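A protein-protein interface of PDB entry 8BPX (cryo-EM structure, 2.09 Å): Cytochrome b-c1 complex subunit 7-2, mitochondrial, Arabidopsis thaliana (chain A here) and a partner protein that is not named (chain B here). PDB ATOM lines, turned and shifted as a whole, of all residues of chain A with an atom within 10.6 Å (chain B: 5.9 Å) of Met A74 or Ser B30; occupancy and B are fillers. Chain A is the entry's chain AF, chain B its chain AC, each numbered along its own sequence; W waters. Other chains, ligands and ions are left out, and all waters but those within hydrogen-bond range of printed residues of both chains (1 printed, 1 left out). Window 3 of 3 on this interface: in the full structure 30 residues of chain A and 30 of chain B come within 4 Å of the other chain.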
ATOM      1  N   ARG A  30     -10.953 -12.863 -14.705  1.00  0.00           N
ATOM      2  CA  ARG A  30     -11.312 -12.950 -13.292  1.00  0.00           C
ATOM      3  C   ARG A  30     -10.144 -13.422 -12.428  1.00  0.00           C
ATOM      4  O   ARG A  30     -10.018 -12.998 -11.275  1.00  0.00           O
ATOM      5  CB  ARG A  30     -12.510 -13.881 -13.119  1.00  0.00           C
ATOM      6  CG  ARG A  30     -13.836 -13.245 -13.464  1.00  0.00           C
ATOM      7  CD  ARG A  30     -14.943 -13.788 -12.596  1.00  0.00           C
ATOM      8  NE  ARG A  30     -15.281 -15.163 -12.939  1.00  0.00           N
ATOM      9  CZ  ARG A  30     -16.224 -15.506 -13.805  1.00  0.00           C
ATOM     10  NH1 ARG A  30     -16.960 -14.597 -14.420  1.00  0.00           N
ATOM     11  NH2 ARG A  30     -16.430 -16.794 -14.061  1.00  0.00           N
ATOM     12  N   TYR A  31      -9.292 -14.297 -12.969  1.00  0.00           N
ATOM     13  CA  TYR A  31      -8.150 -14.888 -12.229  1.00  0.00           C
ATOM     14  C   TYR A  31      -6.816 -14.205 -12.567  1.00  0.00           C
ATOM     15  O   TYR A  31      -5.827 -14.634 -11.999  1.00  0.00           O
ATOM     16  CB  TYR A  31      -8.100 -16.412 -12.418  1.00  0.00           C
ATOM     17  CG  TYR A  31      -9.145 -17.174 -11.653  1.00  0.00           C
ATOM     18  CD1 TYR A  31      -9.081 -17.287 -10.275  1.00  0.00           C
ATOM     19  CD2 TYR A  31     -10.203 -17.777 -12.309  1.00  0.00           C
ATOM     20  CE1 TYR A  31     -10.041 -17.987  -9.566  1.00  0.00           C
ATOM     21  CE2 TYR A  31     -11.172 -18.479 -11.617  1.00  0.00           C
ATOM     22  CZ  TYR A  31     -11.088 -18.586 -10.242  1.00  0.00           C
ATOM     23  OH  TYR A  31     -12.046 -19.269  -9.560  1.00  0.00           O
ATOM     24  N   LEU A  66       0.486 -17.511 -12.002  1.00  0.00           N
ATOM     25  CA  LEU A  66      -0.061 -18.768 -11.508  1.00  0.00           C
ATOM     26  C   LEU A  66      -0.231 -18.744  -9.993  1.00  0.00           C
ATOM     27  O   LEU A  66      -1.255 -19.199  -9.473  1.00  0.00           O
ATOM     28  CB  LEU A  66       0.828 -19.935 -11.934  1.00  0.00           C
ATOM     29  CG  LEU A  66       0.751 -20.296 -13.417  1.00  0.00           C
ATOM     30  CD1 LEU A  66       1.807 -21.325 -13.781  1.00  0.00           C
ATOM     31  CD2 LEU A  66      -0.640 -20.779 -13.789  1.00  0.00           C
ATOM     32  N   MET A  67       0.757 -18.210  -9.271  1.00  0.00           N
ATOM     33  CA  MET A  67       0.647 -18.127  -7.817  1.00  0.00           C
ATOM     34  C   MET A  67      -0.490 -17.200  -7.396  1.00  0.00           C
ATOM     35  O   MET A  67      -1.255 -17.523  -6.481  1.00  0.00           O
ATOM     36  CB  MET A  67       1.968 -17.659  -7.211  1.00  0.00           C
ATOM     37  CG  MET A  67       2.020 -17.784  -5.700  1.00  0.00           C
ATOM     38  SD  MET A  67       3.670 -17.611  -5.005  1.00  0.00           S
ATOM     39  CE  MET A  67       3.318 -17.816  -3.262  1.00  0.00           C
ATOM     40  N   ARG A  68      -0.618 -16.049  -8.060  1.00  0.00           N
ATOM     41  CA  ARG A  68      -1.713 -15.135  -7.758  1.00  0.00           C
ATOM     42  C   ARG A  68      -3.065 -15.796  -8.010  1.00  0.00           C
ATOM     43  O   ARG A  68      -3.986 -15.679  -7.193  1.00  0.00           O
ATOM     44  CB  ARG A  68      -1.559 -13.860  -8.589  1.00  0.00           C
ATOM     45  CG  ARG A  68      -2.704 -12.860  -8.475  1.00  0.00           C
ATOM     46  CD  ARG A  68      -2.376 -11.579  -9.221  1.00  0.00           C
ATOM     47  NE  ARG A  68      -2.440 -11.774 -10.665  1.00  0.00           N
ATOM     48  CZ  ARG A  68      -2.245 -10.824 -11.569  1.00  0.00           C
ATOM     49  NH1 ARG A  68      -1.988  -9.575 -11.217  1.00  0.00           N
ATOM     50  NH2 ARG A  68      -2.306 -11.138 -12.860  1.00  0.00           N
ATOM     51  N   ALA A  69      -3.188 -16.516  -9.128  1.00  0.00           N
ATOM     52  CA  ALA A  69      -4.437 -17.197  -9.445  1.00  0.00           C
ATOM     53  C   ALA A  69      -4.752 -18.284  -8.427  1.00  0.00           C
ATOM     54  O   ALA A  69      -5.903 -18.441  -8.018  1.00  0.00           O
ATOM     55  CB  ALA A  69      -4.375 -17.786 -10.851  1.00  0.00           C
ATOM     56  N   MET A  70      -3.743 -19.055  -8.019  1.00  0.00           N
ATOM     57  CA  MET A  70      -3.967 -20.094  -7.020  1.00  0.00           C
ATOM     58  C   MET A  70      -4.396 -19.487  -5.688  1.00  0.00           C
ATOM     59  O   MET A  70      -5.277 -20.026  -5.012  1.00  0.00           O
ATOM     60  CB  MET A  70      -2.711 -20.948  -6.855  1.00  0.00           C
ATOM     61  CG  MET A  70      -2.554 -22.011  -7.928  1.00  0.00           C
ATOM     62  SD  MET A  70      -1.202 -23.160  -7.607  1.00  0.00           S
ATOM     63  CE  MET A  70      -1.959 -24.246  -6.396  1.00  0.00           C
ATOM     64  N   ASP A  71      -3.802 -18.352  -5.311  1.00  0.00           N
ATOM     65  CA  ASP A  71      -4.210 -17.667  -4.088  1.00  0.00           C
ATOM     66  C   ASP A  71      -5.665 -17.212  -4.171  1.00  0.00           C
ATOM     67  O   ASP A  71      -6.442 -17.403  -3.226  1.00  0.00           O
ATOM     68  CB  ASP A  71      -3.278 -16.484  -3.822  1.00  0.00           C
ATOM     69  CG  ASP A  71      -3.621 -15.741  -2.546  1.00  0.00           C
ATOM     70  OD1 ASP A  71      -3.356 -16.276  -1.451  1.00  0.00           O
ATOM     71  OD2 ASP A  71      -4.153 -14.616  -2.636  1.00  0.00           O
ATOM     72  N   LEU A  72      -6.056 -16.626  -5.305  1.00  0.00           N
ATOM     73  CA  LEU A  72      -7.447 -16.208  -5.479  1.00  0.00           C
ATOM     74  C   LEU A  72      -8.392 -17.406  -5.432  1.00  0.00           C
ATOM     75  O   LEU A  72      -9.442 -17.359  -4.783  1.00  0.00           O
ATOM     76  CB  LEU A  72      -7.612 -15.441  -6.791  1.00  0.00           C
ATOM     77  CG  LEU A  72      -6.847 -14.122  -6.937  1.00  0.00           C
ATOM     78  CD1 LEU A  72      -6.699 -13.745  -8.397  1.00  0.00           C
ATOM     79  CD2 LEU A  72      -7.528 -13.012  -6.164  1.00  0.00           C
ATOM     80  N   SER A  73      -8.018 -18.498  -6.101  1.00  0.00           N
ATOM     81  CA  SER A  73      -8.827 -19.712  -6.104  1.00  0.00           C
ATOM     82  C   SER A  73      -9.006 -20.260  -4.693  1.00  0.00           C
ATOM     83  O   SER A  73     -10.105 -20.672  -4.308  1.00  0.00           O
ATOM     84  CB  SER A  73      -8.176 -20.758  -7.014  1.00  0.00           C
ATOM     85  OG  SER A  73      -9.006 -21.884  -7.192  1.00  0.00           O
ATOM     86  N   MET A  74      -7.928 -20.268  -3.909  1.00  0.00           N
ATOM     87  CA  MET A  74      -8.006 -20.715  -2.523  1.00  0.00           C
ATOM     88  C   MET A  74      -8.914 -19.814  -1.696  1.00  0.00           C
ATOM     89  O   MET A  74      -9.679 -20.299  -0.856  1.00  0.00           O
ATOM     90  CB  MET A  74      -6.609 -20.762  -1.905  1.00  0.00           C
ATOM     91  CG  MET A  74      -6.576 -21.335  -0.501  1.00  0.00           C
ATOM     92  SD  MET A  74      -6.282 -20.079   0.763  1.00  0.00           S
ATOM     93  CE  MET A  74      -4.726 -19.372   0.230  1.00  0.00           C
ATOM     94  N   LYS A  75      -8.843 -18.502  -1.917  1.00  0.00           N
ATOM     95  CA  LYS A  75      -9.612 -17.559  -1.116  1.00  0.00           C
ATOM     96  C   LYS A  75     -11.064 -17.423  -1.557  1.00  0.00           C
ATOM     97  O   LYS A  75     -11.824 -16.720  -0.885  1.00  0.00           O
ATOM     98  CB  LYS A  75      -8.941 -16.182  -1.143  1.00  0.00           C
ATOM     99  CG  LYS A  75      -7.709 -16.073  -0.269  1.00  0.00           C
ATOM    100  CD  LYS A  75      -6.869 -14.869  -0.643  1.00  0.00           C
ATOM    101  CE  LYS A  75      -5.719 -14.672   0.326  1.00  0.00           C
ATOM    102  NZ  LYS A  75      -4.765 -13.636  -0.144  1.00  0.00           N
ATOM    103  N   HIS A  76     -11.512 -18.100  -2.631  1.00  0.00           N
ATOM    104  CA  HIS A  76     -12.850 -17.937  -3.302  1.00  0.00           C
ATOM    105  C   HIS A  76     -13.122 -16.473  -3.717  1.00  0.00           C
ATOM    106  O   HIS A  76     -14.217 -15.969  -3.559  1.00  0.00           O
ATOM    107  CB  HIS A  76     -13.994 -18.564  -2.462  1.00  0.00           C
ATOM    108  CG  HIS A  76     -15.356 -18.525  -3.061  1.00  0.00           C
ATOM    109  ND1 HIS A  76     -16.380 -17.777  -2.509  1.00  0.00           N
ATOM    110  CD2 HIS A  76     -15.880 -19.145  -4.137  1.00  0.00           C
ATOM    111  CE1 HIS A  76     -17.468 -17.933  -3.230  1.00  0.00           C
ATOM    112  NE2 HIS A  76     -17.186 -18.768  -4.229  1.00  0.00           N
ATOM    113  N   GLU A  77     -12.110 -15.810  -4.212  1.00  0.00           N
ATOM    114  CA  GLU A  77     -12.226 -14.414  -4.587  1.00  0.00           C
ATOM    115  C   GLU A  77     -11.624 -14.214  -5.969  1.00  0.00           C
ATOM    116  O   GLU A  77     -10.828 -15.024  -6.447  1.00  0.00           O
ATOM    117  CB  GLU A  77     -11.565 -13.502  -3.539  1.00  0.00           C
ATOM    118  CG  GLU A  77     -10.112 -13.187  -3.775  1.00  0.00           C
ATOM    119  CD  GLU A  77      -9.444 -12.572  -2.553  1.00  0.00           C
ATOM    120  OE1 GLU A  77      -9.948 -12.778  -1.427  1.00  0.00           O
ATOM    121  OE2 GLU A  77      -8.417 -11.883  -2.717  1.00  0.00           O
ATOM    122  N   TYR A  78     -12.178 -13.276  -6.721  1.00  0.00           N
ATOM    123  CA  TYR A  78     -11.609 -12.815  -8.022  1.00  0.00           C
ATOM    124  C   TYR A  78     -10.716 -11.581  -7.828  1.00  0.00           C
ATOM    125  O   TYR A  78     -10.797 -10.956  -6.787  1.00  0.00           O
ATOM    126  CB  TYR A  78     -12.732 -12.544  -9.024  1.00  0.00           C
ATOM    127  CG  TYR A  78     -13.640 -13.710  -9.300  1.00  0.00           C
ATOM    128  CD1 TYR A  78     -13.131 -14.973  -9.564  1.00  0.00           C
ATOM    129  CD2 TYR A  78     -15.013 -13.544  -9.290  1.00  0.00           C
ATOM    130  CE1 TYR A  78     -13.969 -16.043  -9.821  1.00  0.00           C
ATOM    131  CE2 TYR A  78     -15.865 -14.602  -9.539  1.00  0.00           C
ATOM    132  CZ  TYR A  78     -15.340 -15.851  -9.807  1.00  0.00           C
ATOM    133  OH  TYR A  78     -16.192 -16.875 -10.067  1.00  0.00           O
ATOM    134  N   LEU A  79      -9.896 -11.251  -8.828  1.00  0.00           N
ATOM    135  CA  LEU A  79      -9.117 -10.005  -8.880  1.00  0.00           C
ATOM    136  C   LEU A  79     -10.063  -8.814  -8.710  1.00  0.00           C
ATOM    137  O   LEU A  79     -11.162  -8.830  -9.239  1.00  0.00           O
ATOM    138  CB  LEU A  79      -8.444  -9.861 -10.236  1.00  0.00           C
ATOM    139  CG  LEU A  79      -7.042 -10.404 -10.494  1.00  0.00           C
ATOM    140  CD1 LEU A  79      -6.607  -9.937 -11.867  1.00  0.00           C
ATOM    141  CD2 LEU A  79      -6.038  -9.943  -9.451  1.00  0.00           C
ATOM    142  N   THR B  28       0.424 -30.603  -1.646  1.00  0.00           N
ATOM    143  CA  THR B  28      -0.924 -30.614  -2.183  1.00  0.00           C
ATOM    144  C   THR B  28      -1.304 -29.213  -2.642  1.00  0.00           C
ATOM    145  O   THR B  28      -1.015 -28.237  -1.940  1.00  0.00           O
ATOM    146  CB  THR B  28      -1.915 -31.112  -1.117  1.00  0.00           C
ATOM    147  OG1 THR B  28      -1.385 -32.282  -0.479  1.00  0.00           O
ATOM    148  CG2 THR B  28      -3.256 -31.447  -1.726  1.00  0.00           C
ATOM    149  N   PRO B  29      -1.938 -29.075  -3.807  1.00  0.00           N
ATOM    150  CA  PRO B  29      -2.345 -27.740  -4.271  1.00  0.00           C
ATOM    151  C   PRO B  29      -3.307 -27.084  -3.292  1.00  0.00           C
ATOM    152  O   PRO B  29      -4.316 -27.669  -2.898  1.00  0.00           O
ATOM    153  CB  PRO B  29      -3.012 -28.020  -5.623  1.00  0.00           C
ATOM    154  CG  PRO B  29      -2.458 -29.340  -6.047  1.00  0.00           C
ATOM    155  CD  PRO B  29      -2.304 -30.118  -4.780  1.00  0.00           C
ATOM    156  N   SER B  30      -3.000 -25.838  -2.929  1.00  0.00           N
ATOM    157  CA  SER B  30      -3.736 -25.133  -1.889  1.00  0.00           C
ATOM    158  C   SER B  30      -5.178 -24.816  -2.269  1.00  0.00           C
ATOM    159  O   SER B  30      -5.969 -24.485  -1.381  1.00  0.00           O
ATOM    160  CB  SER B  30      -3.009 -23.837  -1.527  1.00  0.00           C
ATOM    161  OG  SER B  30      -3.061 -22.906  -2.590  1.00  0.00           O
ATOM    162  N   ASN B  31      -5.544 -24.910  -3.547  1.00  0.00           N
ATOM    163  CA  ASN B  31      -6.865 -24.508  -4.010  1.00  0.00           C
ATOM    164  C   ASN B  31      -7.792 -25.693  -4.279  1.00  0.00           C
ATOM    165  O   ASN B  31      -8.790 -25.535  -4.987  1.00  0.00           O
ATOM    166  CB  ASN B  31      -6.743 -23.636  -5.263  1.00  0.00           C
ATOM    167  CG  ASN B  31      -6.314 -24.425  -6.487  1.00  0.00           C
ATOM    168  OD1 ASN B  31      -5.530 -25.364  -6.388  1.00  0.00           O
ATOM    169  ND2 ASN B  31      -6.833 -24.048  -7.648  1.00  0.00           N
ATOM    170  N   LEU B  32      -7.484 -26.871  -3.738  1.00  0.00           N
ATOM    171  CA  LEU B  32      -8.384 -28.009  -3.878  1.00  0.00           C
ATOM    172  C   LEU B  32      -9.717 -27.724  -3.196  1.00  0.00           C
ATOM    173  O   LEU B  32      -9.758 -27.233  -2.066  1.00  0.00           O
ATOM    174  CB  LEU B  32      -7.748 -29.269  -3.281  1.00  0.00           C
ATOM    175  CG  LEU B  32      -6.587 -29.923  -4.033  1.00  0.00           C
ATOM    176  CD1 LEU B  32      -6.354 -31.342  -3.527  1.00  0.00           C
ATOM    177  CD2 LEU B  32      -6.812 -29.905  -5.543  1.00  0.00           C
ATOM    178  N   ASP B 223       2.266 -23.115  -5.498  1.00  0.00           N
ATOM    179  CA  ASP B 223       1.390 -22.859  -4.352  1.00  0.00           C
ATOM    180  C   ASP B 223       0.915 -24.154  -3.697  1.00  0.00           C
ATOM    181  O   ASP B 223      -0.282 -24.372  -3.507  1.00  0.00           O
ATOM    182  CB  ASP B 223       0.191 -21.998  -4.743  1.00  0.00           C
ATOM    183  CG  ASP B 223      -0.338 -21.177  -3.575  1.00  0.00           C
ATOM    184  OD1 ASP B 223      -1.304 -20.414  -3.765  1.00  0.00           O
ATOM    185  OD2 ASP B 223       0.211 -21.300  -2.462  1.00  0.00           O
ATOM    186  N   LYS B 224       1.840 -25.040  -3.354  1.00  0.00           N
ATOM    187  CA  LYS B 224       1.462 -26.279  -2.690  1.00  0.00           C
ATOM    188  C   LYS B 224       1.682 -26.189  -1.181  1.00  0.00           C
ATOM    189  O   LYS B 224       2.568 -25.481  -0.701  1.00  0.00           O
ATOM    190  CB  LYS B 224       2.237 -27.459  -3.277  1.00  0.00           C
ATOM    191  CG  LYS B 224       1.659 -27.910  -4.605  1.00  0.00           C
ATOM    192  CD  LYS B 224       2.423 -29.048  -5.227  1.00  0.00           C
ATOM    193  CE  LYS B 224       1.552 -29.768  -6.238  1.00  0.00           C
ATOM    194  NZ  LYS B 224       2.313 -30.725  -7.075  1.00  0.00           N
ATOM    195  N   ILE B 225       0.838 -26.910  -0.436  1.00  0.00           N
ATOM    196  CA  ILE B 225       0.888 -26.960   1.019  1.00  0.00           C
ATOM    197  C   ILE B 225       0.816 -28.418   1.459  1.00  0.00           C
ATOM    198  O   ILE B 225       0.390 -29.299   0.713  1.00  0.00           O
ATOM    199  CB  ILE B 225      -0.246 -26.138   1.678  1.00  0.00           C
ATOM    200  CG1 ILE B 225      -1.618 -26.599   1.169  1.00  0.00           C
ATOM    201  CG2 ILE B 225      -0.052 -24.647   1.430  1.00  0.00           C
ATOM    202  CD1 ILE B 225      -2.787 -26.011   1.924  1.00  0.00           C
ATOM    203  N   PHE B 231      -5.581 -30.329   4.543  1.00  0.00           N
ATOM    204  CA  PHE B 231      -6.521 -31.204   3.869  1.00  0.00           C
ATOM    205  C   PHE B 231      -6.990 -32.336   4.761  1.00  0.00           C
ATOM    206  O   PHE B 231      -8.063 -32.888   4.514  1.00  0.00           O
ATOM    207  CB  PHE B 231      -5.908 -31.699   2.562  1.00  0.00           C
ATOM    208  CG  PHE B 231      -5.732 -30.599   1.570  1.00  0.00           C
ATOM    209  CD1 PHE B 231      -6.833 -30.062   0.921  1.00  0.00           C
ATOM    210  CD2 PHE B 231      -4.489 -30.037   1.347  1.00  0.00           C
ATOM    211  CE1 PHE B 231      -6.686 -29.023   0.033  1.00  0.00           C
ATOM    212  CE2 PHE B 231      -4.339 -28.994   0.459  1.00  0.00           C
ATOM    213  CZ  PHE B 231      -5.439 -28.487  -0.196  1.00  0.00           C
HETATM  214  O   HOH W   1     -10.931 -24.006  -4.470  1.00  0.00           O
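Met A74 touches just these residues of chain B: Ser B30 (3.3 Å) and Asn B31 (3.8 Å). Of chain A, only Met A70 (3.7 Å), Ser A73 (3.1 Å) and Met A74 (3.8 Å) come within 4 Å of Asn B31. No residue of chain A comes within 4 Å of Ile B225. Printed residues of chain B within 4 Å of Met A70: Pro B29, Ser B30, Asn B31 and Asp B223. Printed residues of chain B within 4 Å of Asp A71: Asp B223 (3.6 Å). Of the printed residues of chain B, Met A67 touches Asp B223. Ala A69 touches none of the printed residues of chain B. The nearest residue of chain B that does not touch Met A74 is Asp B223 (5.4 Å). The nearest residue of chain A that does not touch Ser B30 is Asp A71 (5.4 Å).
Water W1 lies within hydrogen-bond range of O of Asn B31 and O of Ser A73.
Among the printed residues, merely in contact across the chains: Met A67 with Asp B223 (3.97 Å), Met A70 with Pro B29 (3.99 Å), Met A70 with Ser B30 (3.95 Å), Met A70 with Asn B31 (3.7 Å), Met A70 with Asp B223 (3.3 Å), Asp A71 with Asp B223 (3.6 Å), Met A74 with Ser B30 (3.3 Å) and Met A74 with Asn B31 (3.8 Å).
Printed residues of chain B that touch a printed residue of chain A: Pro B29, Ser B30, Asn B31 and Asp B223. Hydrophobic or aromatic side chains of chain B that line the printed part of chain A: Pro B29. Printed residues of chain A that touch a printed residue of chain B: Met A67, Met A70, Asp A71, Ser A73 and Met A74. Hydrophobic or aromatic side chains of chain A that line the printed part of chain B: Met A70 and Met A74.
The side-chain amide nitrogen (ND2) of Asn B31 is in hydrogen-bond range of the side-chain hydroxyl (OG) of Ser A73, 3.1 Å away.
O of Asp B223 lies within hydrogen-bond range of N of Ser B30, 3.1 Å away. The side-chain amino group (NZ) of Lys A75 is in salt-bridge range of the side-chain carboxylate (OD2) of Asp A71.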
